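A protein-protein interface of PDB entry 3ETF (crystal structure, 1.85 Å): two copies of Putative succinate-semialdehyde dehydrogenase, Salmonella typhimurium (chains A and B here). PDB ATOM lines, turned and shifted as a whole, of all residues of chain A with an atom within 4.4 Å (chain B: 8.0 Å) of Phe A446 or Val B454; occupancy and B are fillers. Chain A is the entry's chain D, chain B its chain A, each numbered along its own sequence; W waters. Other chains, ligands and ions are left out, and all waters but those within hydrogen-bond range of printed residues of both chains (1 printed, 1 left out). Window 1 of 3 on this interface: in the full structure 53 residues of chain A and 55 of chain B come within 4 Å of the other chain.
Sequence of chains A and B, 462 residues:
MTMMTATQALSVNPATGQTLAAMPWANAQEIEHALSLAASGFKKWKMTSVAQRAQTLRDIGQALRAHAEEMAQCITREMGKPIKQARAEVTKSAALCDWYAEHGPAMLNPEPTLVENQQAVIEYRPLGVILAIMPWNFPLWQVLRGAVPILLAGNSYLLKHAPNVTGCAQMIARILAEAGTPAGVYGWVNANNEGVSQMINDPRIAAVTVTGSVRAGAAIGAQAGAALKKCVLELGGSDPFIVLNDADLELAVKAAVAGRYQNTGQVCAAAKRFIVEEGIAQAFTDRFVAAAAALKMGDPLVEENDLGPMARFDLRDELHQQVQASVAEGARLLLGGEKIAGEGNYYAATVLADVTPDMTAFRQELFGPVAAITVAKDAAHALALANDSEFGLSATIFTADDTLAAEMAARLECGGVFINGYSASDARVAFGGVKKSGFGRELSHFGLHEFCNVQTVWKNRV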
ATOM      1  N   GLY A 415      26.542  22.180 -33.622  1.00  0.00           N
ATOM      2  CA  GLY A 415      26.457  21.856 -32.197  1.00  0.00           C
ATOM      3  C   GLY A 415      27.247  22.769 -31.277  1.00  0.00           C
ATOM      4  O   GLY A 415      27.176  22.626 -30.053  1.00  0.00           O
ATOM      5  N   ALA A 430      29.246  20.827 -23.884  1.00  0.00           N
ATOM      6  CA  ALA A 430      28.948  19.771 -24.873  1.00  0.00           C
ATOM      7  C   ALA A 430      29.780  19.907 -26.153  1.00  0.00           C
ATOM      8  O   ALA A 430      30.070  21.026 -26.621  1.00  0.00           O
ATOM      9  CB  ALA A 430      27.440  19.804 -25.236  1.00  0.00           C
ATOM     10  N   ARG A 441      26.591  13.456 -28.070  1.00  0.00           N
ATOM     11  CA  ARG A 441      27.448  14.517 -27.516  1.00  0.00           C
ATOM     12  C   ARG A 441      28.469  13.943 -26.568  1.00  0.00           C
ATOM     13  O   ARG A 441      28.195  12.952 -25.876  1.00  0.00           O
ATOM     14  CB  ARG A 441      26.608  15.562 -26.776  1.00  0.00           C
ATOM     15  CG  ARG A 441      25.634  16.338 -27.664  1.00  0.00           C
ATOM     16  CD  ARG A 441      26.412  17.285 -28.589  1.00  0.00           C
ATOM     17  NE  ARG A 441      25.574  18.067 -29.513  1.00  0.00           N
ATOM     18  CZ  ARG A 441      25.273  17.698 -30.759  1.00  0.00           C
ATOM     19  NH1 ARG A 441      25.665  16.511 -31.222  1.00  0.00           N
ATOM     20  NH2 ARG A 441      24.558  18.506 -31.537  1.00  0.00           N
ATOM     21  N   LEU A 443      31.541  15.001 -23.484  1.00  0.00           N
ATOM     22  CA  LEU A 443      31.937  15.941 -22.443  1.00  0.00           C
ATOM     23  C   LEU A 443      30.777  16.442 -21.578  1.00  0.00           C
ATOM     24  O   LEU A 443      29.595  16.095 -21.815  1.00  0.00           O
ATOM     25  CB  LEU A 443      32.836  17.065 -23.005  1.00  0.00           C
ATOM     26  CG  LEU A 443      34.132  16.509 -23.620  1.00  0.00           C
ATOM     27  CD1 LEU A 443      34.953  17.626 -24.352  1.00  0.00           C
ATOM     28  CD2 LEU A 443      34.968  15.761 -22.576  1.00  0.00           C
ATOM     29  N   SER A 444      31.124  17.229 -20.551  1.00  0.00           N
ATOM     30  CA  SER A 444      30.167  17.630 -19.523  1.00  0.00           C
ATOM     31  C   SER A 444      29.379  16.387 -19.048  1.00  0.00           C
ATOM     32  O   SER A 444      29.936  15.277 -19.019  1.00  0.00           O
ATOM     33  CB  SER A 444      29.260  18.749 -20.026  1.00  0.00           C
ATOM     34  OG  SER A 444      28.497  19.296 -18.950  1.00  0.00           O
ATOM     35  N   HIS A 445      28.103  16.552 -18.695  1.00  0.00           N
ATOM     36  CA  HIS A 445      27.303  15.394 -18.278  1.00  0.00           C
ATOM     37  C   HIS A 445      26.799  14.576 -19.482  1.00  0.00           C
ATOM     38  O   HIS A 445      26.326  13.442 -19.318  1.00  0.00           O
ATOM     39  CB  HIS A 445      26.137  15.812 -17.364  1.00  0.00           C
ATOM     40  CG  HIS A 445      25.224  16.837 -17.958  1.00  0.00           C
ATOM     41  ND1 HIS A 445      24.091  16.502 -18.673  1.00  0.00           N
ATOM     42  CD2 HIS A 445      25.260  18.187 -17.923  1.00  0.00           C
ATOM     43  CE1 HIS A 445      23.474  17.605 -19.062  1.00  0.00           C
ATOM     44  NE2 HIS A 445      24.160  18.641 -18.612  1.00  0.00           N
ATOM     45  N   PHE A 446      26.912  15.149 -20.676  1.00  0.00           N
ATOM     46  CA  PHE A 446      26.431  14.495 -21.910  1.00  0.00           C
ATOM     47  C   PHE A 446      27.214  13.236 -22.215  1.00  0.00           C
ATOM     48  O   PHE A 446      26.623  12.161 -22.415  1.00  0.00           O
ATOM     49  CB  PHE A 446      26.429  15.481 -23.093  1.00  0.00           C
ATOM     50  CG  PHE A 446      25.675  16.734 -22.794  1.00  0.00           C
ATOM     51  CD1 PHE A 446      24.284  16.775 -22.937  1.00  0.00           C
ATOM     52  CD2 PHE A 446      26.336  17.856 -22.290  1.00  0.00           C
ATOM     53  CE1 PHE A 446      23.571  17.925 -22.610  1.00  0.00           C
ATOM     54  CE2 PHE A 446      25.631  19.016 -21.962  1.00  0.00           C
ATOM     55  CZ  PHE A 446      24.247  19.053 -22.122  1.00  0.00           C
ATOM     56  N   GLY A 447      28.539  13.346 -22.180  1.00  0.00           N
ATOM     57  CA  GLY A 447      29.414  12.225 -22.486  1.00  0.00           C
ATOM     58  C   GLY A 447      29.333  11.153 -21.424  1.00  0.00           C
ATOM     59  O   GLY A 447      29.612   9.986 -21.688  1.00  0.00           O
ATOM     60  N   LEU A 448      28.983  11.545 -20.204  1.00  0.00           N
ATOM     61  CA  LEU A 448      28.820  10.574 -19.155  1.00  0.00           C
ATOM     62  C   LEU A 448      27.495   9.804 -19.325  1.00  0.00           C
ATOM     63  O   LEU A 448      27.462   8.581 -19.182  1.00  0.00           O
ATOM     64  CB  LEU A 448      28.878  11.269 -17.803  1.00  0.00           C
ATOM     65  CG  LEU A 448      28.812  10.399 -16.560  1.00  0.00           C
ATOM     66  CD1 LEU A 448      30.139   9.764 -16.314  1.00  0.00           C
ATOM     67  CD2 LEU A 448      28.463  11.309 -15.402  1.00  0.00           C
ATOM     68  N   HIS A 449      26.422  10.516 -19.650  1.00  0.00           N
ATOM     69  CA  HIS A 449      25.104   9.877 -19.746  1.00  0.00           C
ATOM     70  C   HIS A 449      24.835   9.117 -21.045  1.00  0.00           C
ATOM     71  O   HIS A 449      23.975   8.224 -21.059  1.00  0.00           O
ATOM     72  CB  HIS A 449      23.979  10.881 -19.458  1.00  0.00           C
ATOM     73  CG  HIS A 449      23.970  11.387 -18.049  1.00  0.00           C
ATOM     74  ND1 HIS A 449      23.387  12.584 -17.693  1.00  0.00           N
ATOM     75  CD2 HIS A 449      24.506  10.878 -16.915  1.00  0.00           C
ATOM     76  CE1 HIS A 449      23.542  12.778 -16.394  1.00  0.00           C
ATOM     77  NE2 HIS A 449      24.216  11.758 -15.898  1.00  0.00           N
ATOM     78  N   GLU A 450      25.583   9.412 -22.116  1.00  0.00           N
ATOM     79  CA  GLU A 450      25.369   8.715 -23.393  1.00  0.00           C
ATOM     80  C   GLU A 450      25.466   7.206 -23.232  1.00  0.00           C
ATOM     81  O   GLU A 450      24.747   6.464 -23.922  1.00  0.00           O
ATOM     82  CB  GLU A 450      26.378   9.145 -24.473  1.00  0.00           C
ATOM     83  CG  GLU A 450      26.115  10.527 -25.100  1.00  0.00           C
ATOM     84  CD  GLU A 450      25.015  10.569 -26.183  1.00  0.00           C
ATOM     85  OE1 GLU A 450      24.419   9.515 -26.561  1.00  0.00           O
ATOM     86  OE2 GLU A 450      24.747  11.697 -26.663  1.00  0.00           O
ATOM     87  N   GLU B 111      21.011  25.858 -20.242  1.00  0.00           N
ATOM     88  CA  GLU B 111      21.703  25.405 -19.032  1.00  0.00           C
ATOM     89  C   GLU B 111      22.931  26.264 -18.796  1.00  0.00           C
ATOM     90  O   GLU B 111      23.686  26.506 -19.735  1.00  0.00           O
ATOM     91  CB  GLU B 111      22.258  24.002 -19.223  1.00  0.00           C
ATOM     92  CG  GLU B 111      21.275  22.894 -19.273  1.00  0.00           C
ATOM     93  CD  GLU B 111      21.945  21.536 -19.123  1.00  0.00           C
ATOM     94  OE1 GLU B 111      23.206  21.445 -19.010  1.00  0.00           O
ATOM     95  OE2 GLU B 111      21.197  20.539 -19.114  1.00  0.00           O
ATOM     96  N   PRO B 112      23.138  26.727 -17.552  1.00  0.00           N
ATOM     97  CA  PRO B 112      24.425  27.357 -17.236  1.00  0.00           C
ATOM     98  C   PRO B 112      25.548  26.323 -17.235  1.00  0.00           C
ATOM     99  O   PRO B 112      25.293  25.110 -17.153  1.00  0.00           O
ATOM    100  CB  PRO B 112      24.214  27.920 -15.823  1.00  0.00           C
ATOM    101  CG  PRO B 112      23.075  27.116 -15.236  1.00  0.00           C
ATOM    102  CD  PRO B 112      22.196  26.758 -16.414  1.00  0.00           C
ATOM    103  N   THR B 113      26.789  26.794 -17.347  1.00  0.00           N
ATOM    104  CA  THR B 113      27.938  25.911 -17.306  1.00  0.00           C
ATOM    105  C   THR B 113      28.909  26.458 -16.270  1.00  0.00           C
ATOM    106  O   THR B 113      28.710  27.552 -15.746  1.00  0.00           O
ATOM    107  CB  THR B 113      28.679  25.852 -18.661  1.00  0.00           C
ATOM    108  OG1 THR B 113      29.319  27.111 -18.899  1.00  0.00           O
ATOM    109  CG2 THR B 113      27.714  25.541 -19.821  1.00  0.00           C
ATOM    110  N   VAL B 121      26.716  28.828 -22.289  1.00  0.00           N
ATOM    111  CA  VAL B 121      25.471  28.139 -21.965  1.00  0.00           C
ATOM    112  C   VAL B 121      25.258  26.983 -22.945  1.00  0.00           C
ATOM    113  O   VAL B 121      25.860  26.952 -24.045  1.00  0.00           O
ATOM    114  CB  VAL B 121      24.215  29.091 -22.017  1.00  0.00           C
ATOM    115  CG1 VAL B 121      24.333  30.193 -20.967  1.00  0.00           C
ATOM    116  CG2 VAL B 121      23.976  29.694 -23.420  1.00  0.00           C
ATOM    117  N   ILE B 122      24.430  26.030 -22.537  1.00  0.00           N
ATOM    118  CA  ILE B 122      23.999  24.967 -23.444  1.00  0.00           C
ATOM    119  C   ILE B 122      22.552  25.276 -23.837  1.00  0.00           C
ATOM    120  O   ILE B 122      21.691  25.463 -22.956  1.00  0.00           O
ATOM    121  CB  ILE B 122      24.016  23.577 -22.767  1.00  0.00           C
ATOM    122  CG1 ILE B 122      25.368  23.273 -22.083  1.00  0.00           C
ATOM    123  CG2 ILE B 122      23.648  22.488 -23.794  1.00  0.00           C
ATOM    124  CD1 ILE B 122      26.614  23.445 -22.981  1.00  0.00           C
ATOM    125  N   GLU B 123      22.292  25.351 -25.139  1.00  0.00           N
ATOM    126  CA  GLU B 123      20.937  25.583 -25.657  1.00  0.00           C
ATOM    127  C   GLU B 123      20.411  24.290 -26.249  1.00  0.00           C
ATOM    128  O   GLU B 123      21.184  23.485 -26.767  1.00  0.00           O
ATOM    129  CB  GLU B 123      20.949  26.641 -26.758  1.00  0.00           C
ATOM    130  CG  GLU B 123      21.427  28.010 -26.314  1.00  0.00           C
ATOM    131  CD  GLU B 123      20.337  28.873 -25.701  1.00  0.00           C
ATOM    132  OE1 GLU B 123      19.200  28.378 -25.472  1.00  0.00           O
ATOM    133  OE2 GLU B 123      20.624  30.060 -25.438  1.00  0.00           O
ATOM    134  N   TYR B 124      19.099  24.091 -26.155  1.00  0.00           N
ATOM    135  CA  TYR B 124      18.455  22.920 -26.741  1.00  0.00           C
ATOM    136  C   TYR B 124      17.709  23.363 -27.991  1.00  0.00           C
ATOM    137  O   TYR B 124      16.612  23.907 -27.882  1.00  0.00           O
ATOM    138  CB  TYR B 124      17.498  22.292 -25.714  1.00  0.00           C
ATOM    139  CG  TYR B 124      18.216  21.631 -24.577  1.00  0.00           C
ATOM    140  CD1 TYR B 124      18.652  20.321 -24.682  1.00  0.00           C
ATOM    141  CD2 TYR B 124      18.455  22.318 -23.371  1.00  0.00           C
ATOM    142  CE1 TYR B 124      19.316  19.692 -23.642  1.00  0.00           C
ATOM    143  CE2 TYR B 124      19.126  21.696 -22.311  1.00  0.00           C
ATOM    144  CZ  TYR B 124      19.551  20.385 -22.457  1.00  0.00           C
ATOM    145  OH  TYR B 124      20.225  19.742 -21.442  1.00  0.00           O
ATOM    146  N   ARG B 125      18.310  23.166 -29.170  1.00  0.00           N
ATOM    147  CA  ARG B 125      17.722  23.614 -30.441  1.00  0.00           C
ATOM    148  C   ARG B 125      17.001  22.441 -31.126  1.00  0.00           C
ATOM    149  O   ARG B 125      17.342  21.303 -30.887  1.00  0.00           O
ATOM    150  CB  ARG B 125      18.830  24.076 -31.404  1.00  0.00           C
ATOM    151  CG  ARG B 125      19.875  25.065 -30.808  1.00  0.00           C
ATOM    152  CD  ARG B 125      19.262  26.439 -30.509  1.00  0.00           C
ATOM    153  NE  ARG B 125      20.347  27.404 -30.282  1.00  0.00           N
ATOM    154  CZ  ARG B 125      20.211  28.619 -29.754  1.00  0.00           C
ATOM    155  NH1 ARG B 125      19.019  29.078 -29.345  1.00  0.00           N
ATOM    156  NH2 ARG B 125      21.285  29.384 -29.638  1.00  0.00           N
ATOM    157  N   PRO B 126      16.023  22.716 -31.997  1.00  0.00           N
ATOM    158  CA  PRO B 126      15.470  21.549 -32.717  1.00  0.00           C
ATOM    159  C   PRO B 126      16.441  20.995 -33.754  1.00  0.00           C
ATOM    160  O   PRO B 126      17.386  21.703 -34.145  1.00  0.00           O
ATOM    161  CB  PRO B 126      14.232  22.110 -33.411  1.00  0.00           C
ATOM    162  CG  PRO B 126      14.434  23.556 -33.504  1.00  0.00           C
ATOM    163  CD  PRO B 126      15.338  23.973 -32.343  1.00  0.00           C
ATOM    164  N   LEU B 127      16.229  19.747 -34.168  1.00  0.00           N
ATOM    165  CA  LEU B 127      17.050  19.096 -35.179  1.00  0.00           C
ATOM    166  C   LEU B 127      16.503  19.310 -36.574  1.00  0.00           C
ATOM    167  O   LEU B 127      17.262  19.575 -37.505  1.00  0.00           O
ATOM    168  CB  LEU B 127      17.135  17.580 -34.935  1.00  0.00           C
ATOM    169  CG  LEU B 127      18.145  16.966 -33.994  1.00  0.00           C
ATOM    170  CD1 LEU B 127      17.958  15.439 -33.992  1.00  0.00           C
ATOM    171  CD2 LEU B 127      19.571  17.363 -34.414  1.00  0.00           C
ATOM    172  N   LYS B 230      20.635   9.893 -36.195  1.00  0.00           N
ATOM    173  CA  LYS B 230      20.391   9.266 -34.890  1.00  0.00           C
ATOM    174  C   LYS B 230      19.031   8.572 -34.827  1.00  0.00           C
ATOM    175  O   LYS B 230      18.085   9.003 -35.471  1.00  0.00           O
ATOM    176  CB  LYS B 230      20.445  10.324 -33.785  1.00  0.00           C
ATOM    177  CG  LYS B 230      20.374   9.764 -32.386  1.00  0.00           C
ATOM    178  CD  LYS B 230      20.314  10.876 -31.347  1.00  0.00           C
ATOM    179  CE  LYS B 230      20.015  10.288 -29.985  1.00  0.00           C
ATOM    180  NZ  LYS B 230      20.085  11.275 -28.877  1.00  0.00           N
ATOM    181  N   HIS B 449      14.678  15.669 -25.122  1.00  0.00           N
ATOM    182  CA  HIS B 449      16.055  15.979 -25.527  1.00  0.00           C
ATOM    183  C   HIS B 449      16.656  15.045 -26.573  1.00  0.00           C
ATOM    184  O   HIS B 449      17.630  15.420 -27.235  1.00  0.00           O
ATOM    185  CB  HIS B 449      16.984  16.077 -24.309  1.00  0.00           C
ATOM    186  CG  HIS B 449      16.627  17.187 -23.364  1.00  0.00           C
ATOM    187  ND1 HIS B 449      16.952  17.154 -22.023  1.00  0.00           N
ATOM    188  CD2 HIS B 449      15.966  18.355 -23.561  1.00  0.00           C
ATOM    189  CE1 HIS B 449      16.526  18.264 -21.438  1.00  0.00           C
ATOM    190  NE2 HIS B 449      15.919  19.007 -22.346  1.00  0.00           N
ATOM    191  N   GLU B 450      16.076  13.856 -26.757  1.00  0.00           N
ATOM    192  CA  GLU B 450      16.622  12.904 -27.741  1.00  0.00           C
ATOM    193  C   GLU B 450      16.675  13.522 -29.123  1.00  0.00           C
ATOM    194  O   GLU B 450      17.588  13.226 -29.894  1.00  0.00           O
ATOM    195  CB  GLU B 450      15.798  11.608 -27.801  1.00  0.00           C
ATOM    196  CG  GLU B 450      16.012  10.686 -26.593  1.00  0.00           C
ATOM    197  CD  GLU B 450      17.239   9.774 -26.687  1.00  0.00           C
ATOM    198  OE1 GLU B 450      17.997   9.824 -27.690  1.00  0.00           O
ATOM    199  OE2 GLU B 450      17.447   8.981 -25.741  1.00  0.00           O
ATOM    200  N   PHE B 451      15.710  14.392 -29.435  1.00  0.00           N
ATOM    201  CA  PHE B 451      15.672  15.006 -30.770  1.00  0.00           C
ATOM    202  C   PHE B 451      15.967  16.496 -30.778  1.00  0.00           C
ATOM    203  O   PHE B 451      15.396  17.243 -31.572  1.00  0.00           O
ATOM    204  CB  PHE B 451      14.414  14.611 -31.541  1.00  0.00           C
ATOM    205  CG  PHE B 451      14.323  13.106 -31.741  1.00  0.00           C
ATOM    206  CD1 PHE B 451      15.141  12.470 -32.666  1.00  0.00           C
ATOM    207  CD2 PHE B 451      13.509  12.340 -30.922  1.00  0.00           C
ATOM    208  CE1 PHE B 451      15.118  11.069 -32.824  1.00  0.00           C
ATOM    209  CE2 PHE B 451      13.459  10.924 -31.070  1.00  0.00           C
ATOM    210  CZ  PHE B 451      14.260  10.309 -32.029  1.00  0.00           C
ATOM    211  N   CYS B 452      16.877  16.899 -29.891  1.00  0.00           N
ATOM    212  CA  CYS B 452      17.417  18.241 -29.867  1.00  0.00           C
ATOM    213  C   CYS B 452      18.867  18.238 -30.357  1.00  0.00           C
ATOM    214  O   CYS B 452      19.592  17.234 -30.199  1.00  0.00           O
ATOM    215  CB  CYS B 452      17.410  18.795 -28.424  1.00  0.00           C
ATOM    216  SG  CYS B 452      15.775  19.292 -27.844  1.00  0.00           S
ATOM    217  N   ASN B 453      19.247  19.359 -30.984  1.00  0.00           N
ATOM    218  CA  ASN B 453      20.640  19.705 -31.228  1.00  0.00           C
ATOM    219  C   ASN B 453      21.086  20.415 -29.943  1.00  0.00           C
ATOM    220  O   ASN B 453      20.683  21.555 -29.680  1.00  0.00           O
ATOM    221  CB  ASN B 453      20.735  20.661 -32.417  1.00  0.00           C
ATOM    222  CG  ASN B 453      22.098  21.330 -32.528  1.00  0.00           C
ATOM    223  OD1 ASN B 453      23.078  20.897 -31.909  1.00  0.00           O
ATOM    224  ND2 ASN B 453      22.157  22.410 -33.302  1.00  0.00           N
ATOM    225  N   VAL B 454      21.862  19.717 -29.126  1.00  0.00           N
ATOM    226  CA  VAL B 454      22.369  20.260 -27.859  1.00  0.00           C
ATOM    227  C   VAL B 454      23.530  21.160 -28.299  1.00  0.00           C
ATOM    228  O   VAL B 454      24.516  20.676 -28.856  1.00  0.00           O
ATOM    229  CB  VAL B 454      22.861  19.131 -26.916  1.00  0.00           C
ATOM    230  CG1 VAL B 454      23.682  19.687 -25.742  1.00  0.00           C
ATOM    231  CG2 VAL B 454      21.670  18.307 -26.359  1.00  0.00           C
ATOM    232  N   GLN B 455      23.398  22.464 -28.091  1.00  0.00           N
ATOM    233  CA  GLN B 455      24.326  23.374 -28.718  1.00  0.00           C
ATOM    234  C   GLN B 455      25.042  24.221 -27.687  1.00  0.00           C
ATOM    235  O   GLN B 455      24.392  24.939 -26.936  1.00  0.00           O
ATOM    236  CB  GLN B 455      23.575  24.275 -29.701  1.00  0.00           C
ATOM    237  CG  GLN B 455      24.502  25.212 -30.514  1.00  0.00           C
ATOM    238  CD  GLN B 455      23.751  26.277 -31.241  1.00  0.00           C
ATOM    239  OE1 GLN B 455      23.154  27.163 -30.618  1.00  0.00           O
ATOM    240  NE2 GLN B 455      23.747  26.199 -32.578  1.00  0.00           N
ATOM    241  N   THR B 456      26.366  24.127 -27.649  1.00  0.00           N
ATOM    242  CA  THR B 456      27.152  25.005 -26.775  1.00  0.00           C
ATOM    243  C   THR B 456      27.222  26.395 -27.409  1.00  0.00           C
ATOM    244  O   THR B 456      27.481  26.519 -28.603  1.00  0.00           O
ATOM    245  CB  THR B 456      28.600  24.445 -26.614  1.00  0.00           C
ATOM    246  OG1 THR B 456      28.544  23.234 -25.842  1.00  0.00           O
ATOM    247  CG2 THR B 456      29.511  25.464 -25.906  1.00  0.00           C
ATOM    248  N   VAL B 457      26.987  27.449 -26.627  1.00  0.00           N
ATOM    249  CA  VAL B 457      27.158  28.806 -27.146  1.00  0.00           C
ATOM    250  C   VAL B 457      28.112  29.487 -26.166  1.00  0.00           C
ATOM    251  O   VAL B 457      27.770  29.667 -25.008  1.00  0.00           O
ATOM    252  CB  VAL B 457      25.818  29.594 -27.267  1.00  0.00           C
ATOM    253  CG1 VAL B 457      26.089  30.996 -27.763  1.00  0.00           C
ATOM    254  CG2 VAL B 457      24.841  28.874 -28.213  1.00  0.00           C
HETATM  255  O   HOH W   1      22.263  12.483 -28.260  1.00  0.00           O
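OE1 of Glu B111 is in hydrogen-bond range of NE2 of His A445 (3.0 Å). The side-chain hydroxyl (OG1) of Thr B456 lies within hydrogen-bond range of the backbone carbonyl oxygen (O) of Ala A430 (2.8 Å). N of Thr B456 lies within hydrogen-bond range of O of Gly A415 (2.9 Å). OD1 of Asn B453 sits at hydrogen-bond distance from NH2 of Arg A441 (2.8 Å). The guanidinium group (NE) of Arg A441 lies within hydrogen-bond range of the backbone carbonyl oxygen (O) of Val B454 (2.9 Å).
OE2 of Glu B111 is in hydrogen-bond range of OH of Tyr B124. The side-chain carboxylate of Glu A450 lies within hydrogen-bond range of the backbone NH of Arg A441 (2.9 Å). The backbone carbonyl oxygen (O) of Arg B125 is in hydrogen-bond range of the backbone NH (N) of Asn B453, 2.7 Å away. OE1 of Gln B455 is in hydrogen-bond range of NE of Arg B125 (2.8 Å). O of Glu B123 sits at hydrogen-bond distance from N of Gln B455 (2.8 Å). The backbone NH of Glu B111 sits at hydrogen-bond distance from the backbone carbonyl oxygen of Ile B122, at 2.8 Å.
Gly A415 touches Asn B453. O of Val B454 touches O of Gly A415, 3.5 Å away. Gly A415 touches Gln B455 (O to CA, 3.2 Å). Ile B122 touches Ala A430. Val B454 touches Ala A430 (CG1 to CB, 3.8 Å). Ile B122 touches Phe A446 (CG2 to CZ, 3.9 Å). CE1 of Phe A446 touches OH of Tyr B124 (3.98 Å). Phe A446 touches Val B454 (CE1 to CG1, 3.6 Å).
Printed residues of chain B within 4 Å of Phe A446: Ile B122 (3.9 Å), Tyr B124 (3.98 Å) and Val B454 (3.6 Å). Val B454 touches just these residues of chain A: Gly A415, Ala A430, Arg A441 and Phe A446. No residue of chain B comes within 4 Å of Gly A447. Printed residues of chain A within 4 Å of Glu B111: His A445 (3.0 Å). Printed residues of chain A within 4 Å of Asn B453: Gly A415 and Arg A441. Of the printed residues of chain B, His A445 touches Glu B111 (3.0 Å). Printed residues of chain B within 4 Å of Gly A415: Asn B453 (3.5 Å), Val B454 (3.5 Å), Gln B455 (3.2 Å) and Thr B456 (2.9 Å). Of the printed residues of chain A, Thr B456 touches Gly A415 and Ala A430. Phe B451 touches none of the printed residues of chain A. The nearest printed residue of chain A that does not touch Val B454 is His A445 (7.0 Å).
Of the 20 printed residues of chain B, 7 touch a printed residue of chain A. Hydrophobic or aromatic side chains of chain B that line the printed part of chain A: Ile B122, Tyr B124 and Val B454. Of the 11 printed residues of chain A, 5 touch a printed residue of chain B. Hydrophobic or aromatic side chains of chain A within 4 Å of the printed part of chain B: Ala A430, His A445 and Phe A446. Among the printed residues, 13 pairs touch across the chains. Among the printed residues, no Asp or Glu carboxylate lies within 4 Å of a Lys or Arg side-chain nitrogen of the other chain.
2 positions are printed for both chains.
Water W1 bridges the side-chain amino group (NZ) of Lys B230 (2.6 Å) and the side-chain carboxylate (OE2) of Glu A450 (3.1 Å).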
